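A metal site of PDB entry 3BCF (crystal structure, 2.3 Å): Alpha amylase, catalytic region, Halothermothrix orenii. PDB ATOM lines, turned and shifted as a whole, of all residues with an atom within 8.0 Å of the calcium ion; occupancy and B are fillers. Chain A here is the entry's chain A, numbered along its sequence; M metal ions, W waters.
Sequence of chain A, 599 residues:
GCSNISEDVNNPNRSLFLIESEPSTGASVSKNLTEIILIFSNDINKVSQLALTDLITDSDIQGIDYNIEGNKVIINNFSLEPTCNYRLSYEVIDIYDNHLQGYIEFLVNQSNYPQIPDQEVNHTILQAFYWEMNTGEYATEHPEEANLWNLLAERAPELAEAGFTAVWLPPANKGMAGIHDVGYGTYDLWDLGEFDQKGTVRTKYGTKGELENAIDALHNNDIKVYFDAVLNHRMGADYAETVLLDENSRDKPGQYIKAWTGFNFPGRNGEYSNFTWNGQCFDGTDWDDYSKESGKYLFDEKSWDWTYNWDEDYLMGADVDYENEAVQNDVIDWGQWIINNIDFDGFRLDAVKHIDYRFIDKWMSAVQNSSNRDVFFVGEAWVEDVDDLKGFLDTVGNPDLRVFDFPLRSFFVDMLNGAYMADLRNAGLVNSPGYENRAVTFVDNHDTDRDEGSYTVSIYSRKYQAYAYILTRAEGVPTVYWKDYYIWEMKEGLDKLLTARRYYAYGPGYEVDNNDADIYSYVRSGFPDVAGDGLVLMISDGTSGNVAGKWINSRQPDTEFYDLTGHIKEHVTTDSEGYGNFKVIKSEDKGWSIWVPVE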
ATOM      1  N   GLN A 280      32.440  12.188 -28.139  1.00  0.00           N
ATOM      2  CA  GLN A 280      31.456  12.485 -27.109  1.00  0.00           C
ATOM      3  C   GLN A 280      30.246  13.259 -27.643  1.00  0.00           C
ATOM      4  O   GLN A 280      29.265  13.565 -26.915  1.00  0.00           O
ATOM      5  CB  GLN A 280      32.127  13.279 -25.955  1.00  0.00           C
ATOM      6  CG  GLN A 280      33.176  12.466 -25.080  1.00  0.00           C
ATOM      7  CD  GLN A 280      32.491  11.368 -24.207  1.00  0.00           C
ATOM      8  OE1 GLN A 280      32.813  10.177 -24.333  1.00  0.00           O
ATOM      9  NE2 GLN A 280      31.490  11.767 -23.371  1.00  0.00           N
ATOM     10  N   CYS A 281      30.378  13.637 -28.917  1.00  0.00           N
ATOM     11  CA  CYS A 281      29.290  14.169 -29.692  1.00  0.00           C
ATOM     12  C   CYS A 281      28.372  13.103 -30.331  1.00  0.00           C
ATOM     13  O   CYS A 281      27.381  13.455 -30.948  1.00  0.00           O
ATOM     14  CB  CYS A 281      29.818  15.092 -30.786  1.00  0.00           C
ATOM     15  SG  CYS A 281      30.646  16.519 -30.149  1.00  0.00           S
ATOM     16  N   PHE A 282      28.667  11.833 -30.138  1.00  0.00           N
ATOM     17  CA  PHE A 282      27.992  10.757 -30.850  1.00  0.00           C
ATOM     18  C   PHE A 282      27.653   9.653 -29.890  1.00  0.00           C
ATOM     19  O   PHE A 282      28.294   9.481 -28.885  1.00  0.00           O
ATOM     20  CB  PHE A 282      28.896  10.189 -31.970  1.00  0.00           C
ATOM     21  CG  PHE A 282      29.231  11.194 -33.035  1.00  0.00           C
ATOM     22  CD1 PHE A 282      30.552  11.654 -33.198  1.00  0.00           C
ATOM     23  CD2 PHE A 282      28.210  11.691 -33.877  1.00  0.00           C
ATOM     24  CE1 PHE A 282      30.852  12.598 -34.183  1.00  0.00           C
ATOM     25  CE2 PHE A 282      28.482  12.625 -34.867  1.00  0.00           C
ATOM     26  CZ  PHE A 282      29.814  13.089 -35.038  1.00  0.00           C
ATOM     27  N   ASP A 283      26.580   8.922 -30.185  1.00  0.00           N
ATOM     28  CA  ASP A 283      26.163   7.817 -29.337  1.00  0.00           C
ATOM     29  C   ASP A 283      26.814   6.613 -29.848  1.00  0.00           C
ATOM     30  O   ASP A 283      27.040   5.715 -29.110  1.00  0.00           O
ATOM     31  CB  ASP A 283      24.658   7.621 -29.361  1.00  0.00           C
ATOM     32  CG  ASP A 283      23.911   8.569 -28.413  1.00  0.00           C
ATOM     33  OD1 ASP A 283      24.466   8.856 -27.342  1.00  0.00           O
ATOM     34  OD2 ASP A 283      22.720   9.009 -28.731  1.00  0.00           O
ATOM     35  N   GLY A 284      27.097   6.562 -31.126  1.00  0.00           N
ATOM     36  CA  GLY A 284      27.811   5.419 -31.657  1.00  0.00           C
ATOM     37  C   GLY A 284      28.019   5.445 -33.145  1.00  0.00           C
ATOM     38  O   GLY A 284      27.859   6.449 -33.803  1.00  0.00           O
ATOM     39  N   LEU A 298      27.716   0.973 -29.644  1.00  0.00           N
ATOM     40  CA  LEU A 298      27.342   1.980 -28.686  1.00  0.00           C
ATOM     41  C   LEU A 298      28.564   2.308 -27.831  1.00  0.00           C
ATOM     42  O   LEU A 298      29.151   1.412 -27.236  1.00  0.00           O
ATOM     43  CB  LEU A 298      26.192   1.472 -27.841  1.00  0.00           C
ATOM     44  CG  LEU A 298      25.842   2.417 -26.719  1.00  0.00           C
ATOM     45  CD1 LEU A 298      25.390   3.709 -27.277  1.00  0.00           C
ATOM     46  CD2 LEU A 298      24.768   1.692 -25.810  1.00  0.00           C
ATOM     47  N   GLU A 301      29.189   4.753 -21.778  1.00  0.00           N
ATOM     48  CA  GLU A 301      28.365   5.758 -21.052  1.00  0.00           C
ATOM     49  C   GLU A 301      27.403   6.586 -21.881  1.00  0.00           C
ATOM     50  O   GLU A 301      26.726   7.506 -21.376  1.00  0.00           O
ATOM     51  CB  GLU A 301      29.272   6.627 -20.148  1.00  0.00           C
ATOM     52  CG  GLU A 301      30.183   5.700 -19.246  1.00  0.00           C
ATOM     53  CD  GLU A 301      31.001   6.470 -18.208  1.00  0.00           C
ATOM     54  OE1 GLU A 301      31.514   5.779 -17.273  1.00  0.00           O
ATOM     55  OE2 GLU A 301      31.113   7.734 -18.334  1.00  0.00           O
ATOM     56  N   LYS A 302      27.288   6.259 -23.151  1.00  0.00           N
ATOM     57  CA  LYS A 302      26.208   6.820 -23.935  1.00  0.00           C
ATOM     58  C   LYS A 302      24.970   5.880 -23.939  1.00  0.00           C
ATOM     59  O   LYS A 302      25.081   4.626 -23.862  1.00  0.00           O
ATOM     60  CB  LYS A 302      26.659   7.062 -25.349  1.00  0.00           C
ATOM     61  CG  LYS A 302      27.791   7.988 -25.498  1.00  0.00           C
ATOM     62  CD  LYS A 302      27.435   9.394 -25.060  1.00  0.00           C
ATOM     63  CE  LYS A 302      28.256  10.358 -25.822  1.00  0.00           C
ATOM     64  NZ  LYS A 302      28.077  11.701 -25.300  1.00  0.00           N
ATOM     65  N   SER A 303      23.797   6.510 -24.035  1.00  0.00           N
ATOM     66  CA  SER A 303      22.533   5.805 -24.294  1.00  0.00           C
ATOM     67  C   SER A 303      21.887   6.339 -25.577  1.00  0.00           C
ATOM     68  O   SER A 303      21.959   7.580 -25.886  1.00  0.00           O
ATOM     69  CB  SER A 303      21.587   6.015 -23.129  1.00  0.00           C
ATOM     70  OG  SER A 303      21.449   7.391 -23.008  1.00  0.00           O
ATOM     71  N   TRP A 304      21.327   5.391 -26.338  1.00  0.00           N
ATOM     72  CA  TRP A 304      20.589   5.665 -27.506  1.00  0.00           C
ATOM     73  C   TRP A 304      19.447   6.616 -27.066  1.00  0.00           C
ATOM     74  O   TRP A 304      18.890   6.449 -25.962  1.00  0.00           O
ATOM     75  CB  TRP A 304      19.993   4.372 -28.028  1.00  0.00           C
ATOM     76  CG  TRP A 304      21.004   3.394 -28.612  1.00  0.00           C
ATOM     77  CD1 TRP A 304      21.069   2.082 -28.348  1.00  0.00           C
ATOM     78  CD2 TRP A 304      22.034   3.673 -29.551  1.00  0.00           C
ATOM     79  NE1 TRP A 304      22.098   1.515 -29.047  1.00  0.00           N
ATOM     80  CE2 TRP A 304      22.701   2.480 -29.796  1.00  0.00           C
ATOM     81  CE3 TRP A 304      22.466   4.819 -30.214  1.00  0.00           C
ATOM     82  CZ2 TRP A 304      23.767   2.401 -30.654  1.00  0.00           C
ATOM     83  CZ3 TRP A 304      23.508   4.747 -31.050  1.00  0.00           C
ATOM     84  CH2 TRP A 304      24.139   3.555 -31.303  1.00  0.00           C
ATOM     85  N   ASP A 305      19.202   7.637 -27.882  1.00  0.00           N
ATOM     86  CA  ASP A 305      18.287   8.678 -27.553  1.00  0.00           C
ATOM     87  C   ASP A 305      16.878   8.189 -27.685  1.00  0.00           C
ATOM     88  O   ASP A 305      16.632   7.232 -28.390  1.00  0.00           O
ATOM     89  CB  ASP A 305      18.471   9.899 -28.475  1.00  0.00           C
ATOM     90  CG  ASP A 305      19.889  10.468 -28.421  1.00  0.00           C
ATOM     91  OD1 ASP A 305      20.420  10.503 -27.277  1.00  0.00           O
ATOM     92  OD2 ASP A 305      20.414  10.871 -29.498  1.00  0.00           O
ATOM     93  N   TRP A 306      15.960   8.893 -27.024  1.00  0.00           N
ATOM     94  CA  TRP A 306      14.525   8.530 -27.038  1.00  0.00           C
ATOM     95  C   TRP A 306      13.867   8.675 -28.402  1.00  0.00           C
ATOM     96  O   TRP A 306      13.819   9.742 -28.992  1.00  0.00           O
ATOM     97  CB  TRP A 306      13.740   9.367 -26.028  1.00  0.00           C
ATOM     98  CG  TRP A 306      14.096   9.158 -24.540  1.00  0.00           C
ATOM     99  CD1 TRP A 306      15.220   8.566 -24.017  1.00  0.00           C
ATOM    100  CD2 TRP A 306      13.320   9.595 -23.411  1.00  0.00           C
ATOM    101  NE1 TRP A 306      15.187   8.612 -22.641  1.00  0.00           N
ATOM    102  CE2 TRP A 306      14.028   9.250 -22.248  1.00  0.00           C
ATOM    103  CE3 TRP A 306      12.093  10.251 -23.274  1.00  0.00           C
ATOM    104  CZ2 TRP A 306      13.537   9.544 -20.980  1.00  0.00           C
ATOM    105  CZ3 TRP A 306      11.621  10.525 -22.030  1.00  0.00           C
ATOM    106  CH2 TRP A 306      12.328  10.178 -20.904  1.00  0.00           C
ATOM    107  N   ASP A 313      17.122   4.910 -32.767  1.00  0.00           N
ATOM    108  CA  ASP A 313      18.078   6.070 -32.808  1.00  0.00           C
ATOM    109  C   ASP A 313      19.168   5.703 -33.840  1.00  0.00           C
ATOM    110  O   ASP A 313      19.405   6.489 -34.786  1.00  0.00           O
ATOM    111  CB  ASP A 313      18.659   6.368 -31.399  1.00  0.00           C
ATOM    112  CG  ASP A 313      19.538   7.624 -31.379  1.00  0.00           C
ATOM    113  OD1 ASP A 313      19.516   8.421 -32.346  1.00  0.00           O
ATOM    114  OD2 ASP A 313      20.292   7.816 -30.371  1.00  0.00           O
ATOM    115  N   ASP A 319      26.318   8.381 -35.176  1.00  0.00           N
ATOM    116  CA  ASP A 319      25.049   8.831 -34.675  1.00  0.00           C
ATOM    117  C   ASP A 319      25.107   9.987 -33.667  1.00  0.00           C
ATOM    118  O   ASP A 319      25.659   9.854 -32.561  1.00  0.00           O
ATOM    119  CB  ASP A 319      24.298   7.671 -34.013  1.00  0.00           C
ATOM    120  CG  ASP A 319      22.790   8.042 -33.760  1.00  0.00           C
ATOM    121  OD1 ASP A 319      22.069   8.055 -34.819  1.00  0.00           O
ATOM    122  OD2 ASP A 319      22.390   8.242 -32.549  1.00  0.00           O
ATOM    123  N   VAL A 320      24.503  11.120 -34.036  1.00  0.00           N
ATOM    124  CA  VAL A 320      24.494  12.300 -33.135  1.00  0.00           C
ATOM    125  C   VAL A 320      23.862  11.986 -31.786  1.00  0.00           C
ATOM    126  O   VAL A 320      22.954  11.173 -31.748  1.00  0.00           O
ATOM    127  CB  VAL A 320      23.868  13.505 -33.830  1.00  0.00           C
ATOM    128  CG1 VAL A 320      23.935  14.759 -32.963  1.00  0.00           C
ATOM    129  CG2 VAL A 320      24.652  13.675 -35.149  1.00  0.00           C
ATOM    130  N   ASP A 321      24.466  12.491 -30.692  1.00  0.00           N
ATOM    131  CA  ASP A 321      23.972  12.291 -29.370  1.00  0.00           C
ATOM    132  C   ASP A 321      23.175  13.525 -29.016  1.00  0.00           C
ATOM    133  O   ASP A 321      23.770  14.506 -28.601  1.00  0.00           O
ATOM    134  CB  ASP A 321      25.088  12.123 -28.353  1.00  0.00           C
ATOM    135  CG  ASP A 321      24.542  11.970 -26.890  1.00  0.00           C
ATOM    136  OD1 ASP A 321      23.279  11.932 -26.729  1.00  0.00           O
ATOM    137  OD2 ASP A 321      25.395  11.860 -25.934  1.00  0.00           O
ATOM    138  N   TYR A 322      21.874  13.535 -29.235  1.00  0.00           N
ATOM    139  CA  TYR A 322      21.094  14.739 -28.936  1.00  0.00           C
ATOM    140  C   TYR A 322      20.795  14.890 -27.467  1.00  0.00           C
ATOM    141  O   TYR A 322      20.149  15.820 -27.062  1.00  0.00           O
ATOM    142  CB  TYR A 322      19.828  14.860 -29.832  1.00  0.00           C
ATOM    143  CG  TYR A 322      20.193  15.327 -31.232  1.00  0.00           C
ATOM    144  CD1 TYR A 322      20.182  14.428 -32.317  1.00  0.00           C
ATOM    145  CD2 TYR A 322      20.702  16.639 -31.445  1.00  0.00           C
ATOM    146  CE1 TYR A 322      20.592  14.852 -33.626  1.00  0.00           C
ATOM    147  CE2 TYR A 322      21.140  17.048 -32.748  1.00  0.00           C
ATOM    148  CZ  TYR A 322      21.043  16.169 -33.812  1.00  0.00           C
ATOM    149  OH  TYR A 322      21.449  16.604 -35.035  1.00  0.00           O
ATOM    150  N   GLU A 323      21.302  14.006 -26.631  1.00  0.00           N
ATOM    151  CA  GLU A 323      21.407  14.326 -25.197  1.00  0.00           C
ATOM    152  C   GLU A 323      22.536  15.353 -24.853  1.00  0.00           C
ATOM    153  O   GLU A 323      22.404  16.103 -23.859  1.00  0.00           O
ATOM    154  CB  GLU A 323      21.472  13.048 -24.375  1.00  0.00           C
ATOM    155  CG  GLU A 323      20.160  12.266 -24.614  1.00  0.00           C
ATOM    156  CD  GLU A 323      20.196  10.833 -24.248  1.00  0.00           C
ATOM    157  OE1 GLU A 323      21.222  10.155 -24.507  1.00  0.00           O
ATOM    158  OE2 GLU A 323      19.169  10.351 -23.703  1.00  0.00           O
ATOM    159  N   ASN A 324      23.503  15.506 -25.759  1.00  0.00           N
ATOM    160  CA  ASN A 324      24.672  16.383 -25.565  1.00  0.00           C
ATOM    161  C   ASN A 324      24.334  17.847 -25.864  1.00  0.00           C
ATOM    162  O   ASN A 324      23.931  18.200 -26.951  1.00  0.00           O
ATOM    163  CB  ASN A 324      25.879  15.838 -26.412  1.00  0.00           C
ATOM    164  CG  ASN A 324      27.121  16.709 -26.381  1.00  0.00           C
ATOM    165  OD1 ASN A 324      27.027  17.951 -26.383  1.00  0.00           O
ATOM    166  ND2 ASN A 324      28.301  16.075 -26.518  1.00  0.00           N
ATOM    167  N   ASP A 356      16.142  11.944 -31.611  1.00  0.00           N
ATOM    168  CA  ASP A 356      15.533  12.130 -30.369  1.00  0.00           C
ATOM    169  C   ASP A 356      14.199  12.934 -30.457  1.00  0.00           C
ATOM    170  O   ASP A 356      14.150  14.132 -30.739  1.00  0.00           O
ATOM    171  CB  ASP A 356      16.524  12.854 -29.474  1.00  0.00           C
ATOM    172  CG  ASP A 356      16.068  12.907 -28.029  1.00  0.00           C
ATOM    173  OD1 ASP A 356      14.850  13.263 -27.717  1.00  0.00           O
ATOM    174  OD2 ASP A 356      16.988  12.616 -27.205  1.00  0.00           O
ATOM    175  N   ARG A 358      12.433  14.375 -28.333  1.00  0.00           N
ATOM    176  CA  ARG A 358      12.474  15.562 -27.462  1.00  0.00           C
ATOM    177  C   ARG A 358      13.330  16.637 -28.144  1.00  0.00           C
ATOM    178  O   ARG A 358      13.035  17.819 -27.989  1.00  0.00           O
ATOM    179  CB  ARG A 358      13.037  15.264 -26.059  1.00  0.00           C
ATOM    180  CG  ARG A 358      12.404  14.058 -25.238  1.00  0.00           C
ATOM    181  CD  ARG A 358      13.408  13.530 -24.112  1.00  0.00           C
ATOM    182  NE  ARG A 358      14.608  12.846 -24.718  1.00  0.00           N
ATOM    183  CZ  ARG A 358      15.579  12.279 -24.026  1.00  0.00           C
ATOM    184  NH1 ARG A 358      15.510  12.303 -22.745  1.00  0.00           N
ATOM    185  NH2 ARG A 358      16.642  11.664 -24.625  1.00  0.00           N
HETATM  186 CA    CA M   1      22.457   9.764 -26.411  1.00  0.00          CA
HETATM  187  O   HOH W   1      24.076   9.661 -24.689  1.00  0.00           O
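The guanidinium group of Arg 358 lies within salt-bridge range of the side-chain carboxylate of Glu 323 (3.0 Å).
The side-chain carboxylate (OD2) of Asp 305 is in hydrogen-bond range of the backbone NH (N) of Tyr 322, 3.0 Å away.
N of Asp 305 lies within hydrogen-bond range of OD2 of Asp 313.
The side-chain carboxylate (OD2) of Asp 321 is in salt-bridge range of the side-chain amino group (NZ) of Lys 302 (2.8 Å).
The backbone NH (N) of Asp 321 sits at hydrogen-bond distance from the backbone carbonyl oxygen (O) of Cys 281, 3.1 Å away.
N of Asp 283 is in hydrogen-bond range of O of Asp 319.
Five residues have an atom within 4 Å of the calcium ion: Asp 283, Ser 303, Asp 305, Asp 321 and Glu 323.
The nearest printed residue that does not touch the calcium ion is Trp 304 (4.4 Å).
The backbone carbonyl oxygen (O) of Ser 303 binds the calcium ion (2.3 Å).
OE1 of Glu 323 is bound to the calcium ion.
The calcium ion is bound by OD1 of Asp 305 (2.3 Å).
The calcium ion is bound by OD1 of Asp 321.
The calcium ion is bound by water W1, 2.4 Å away.
The side-chain carboxylate (OD1) of Asp 283 binds the calcium ion (2.4 Å).
OD2 of Asp 283 is bound to the calcium ion, at 2.5 Å.
Water W1 lies within hydrogen-bond range of the side-chain carboxylate (OD2) of Asp 321 and the backbone NH (N) of Ser 303.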
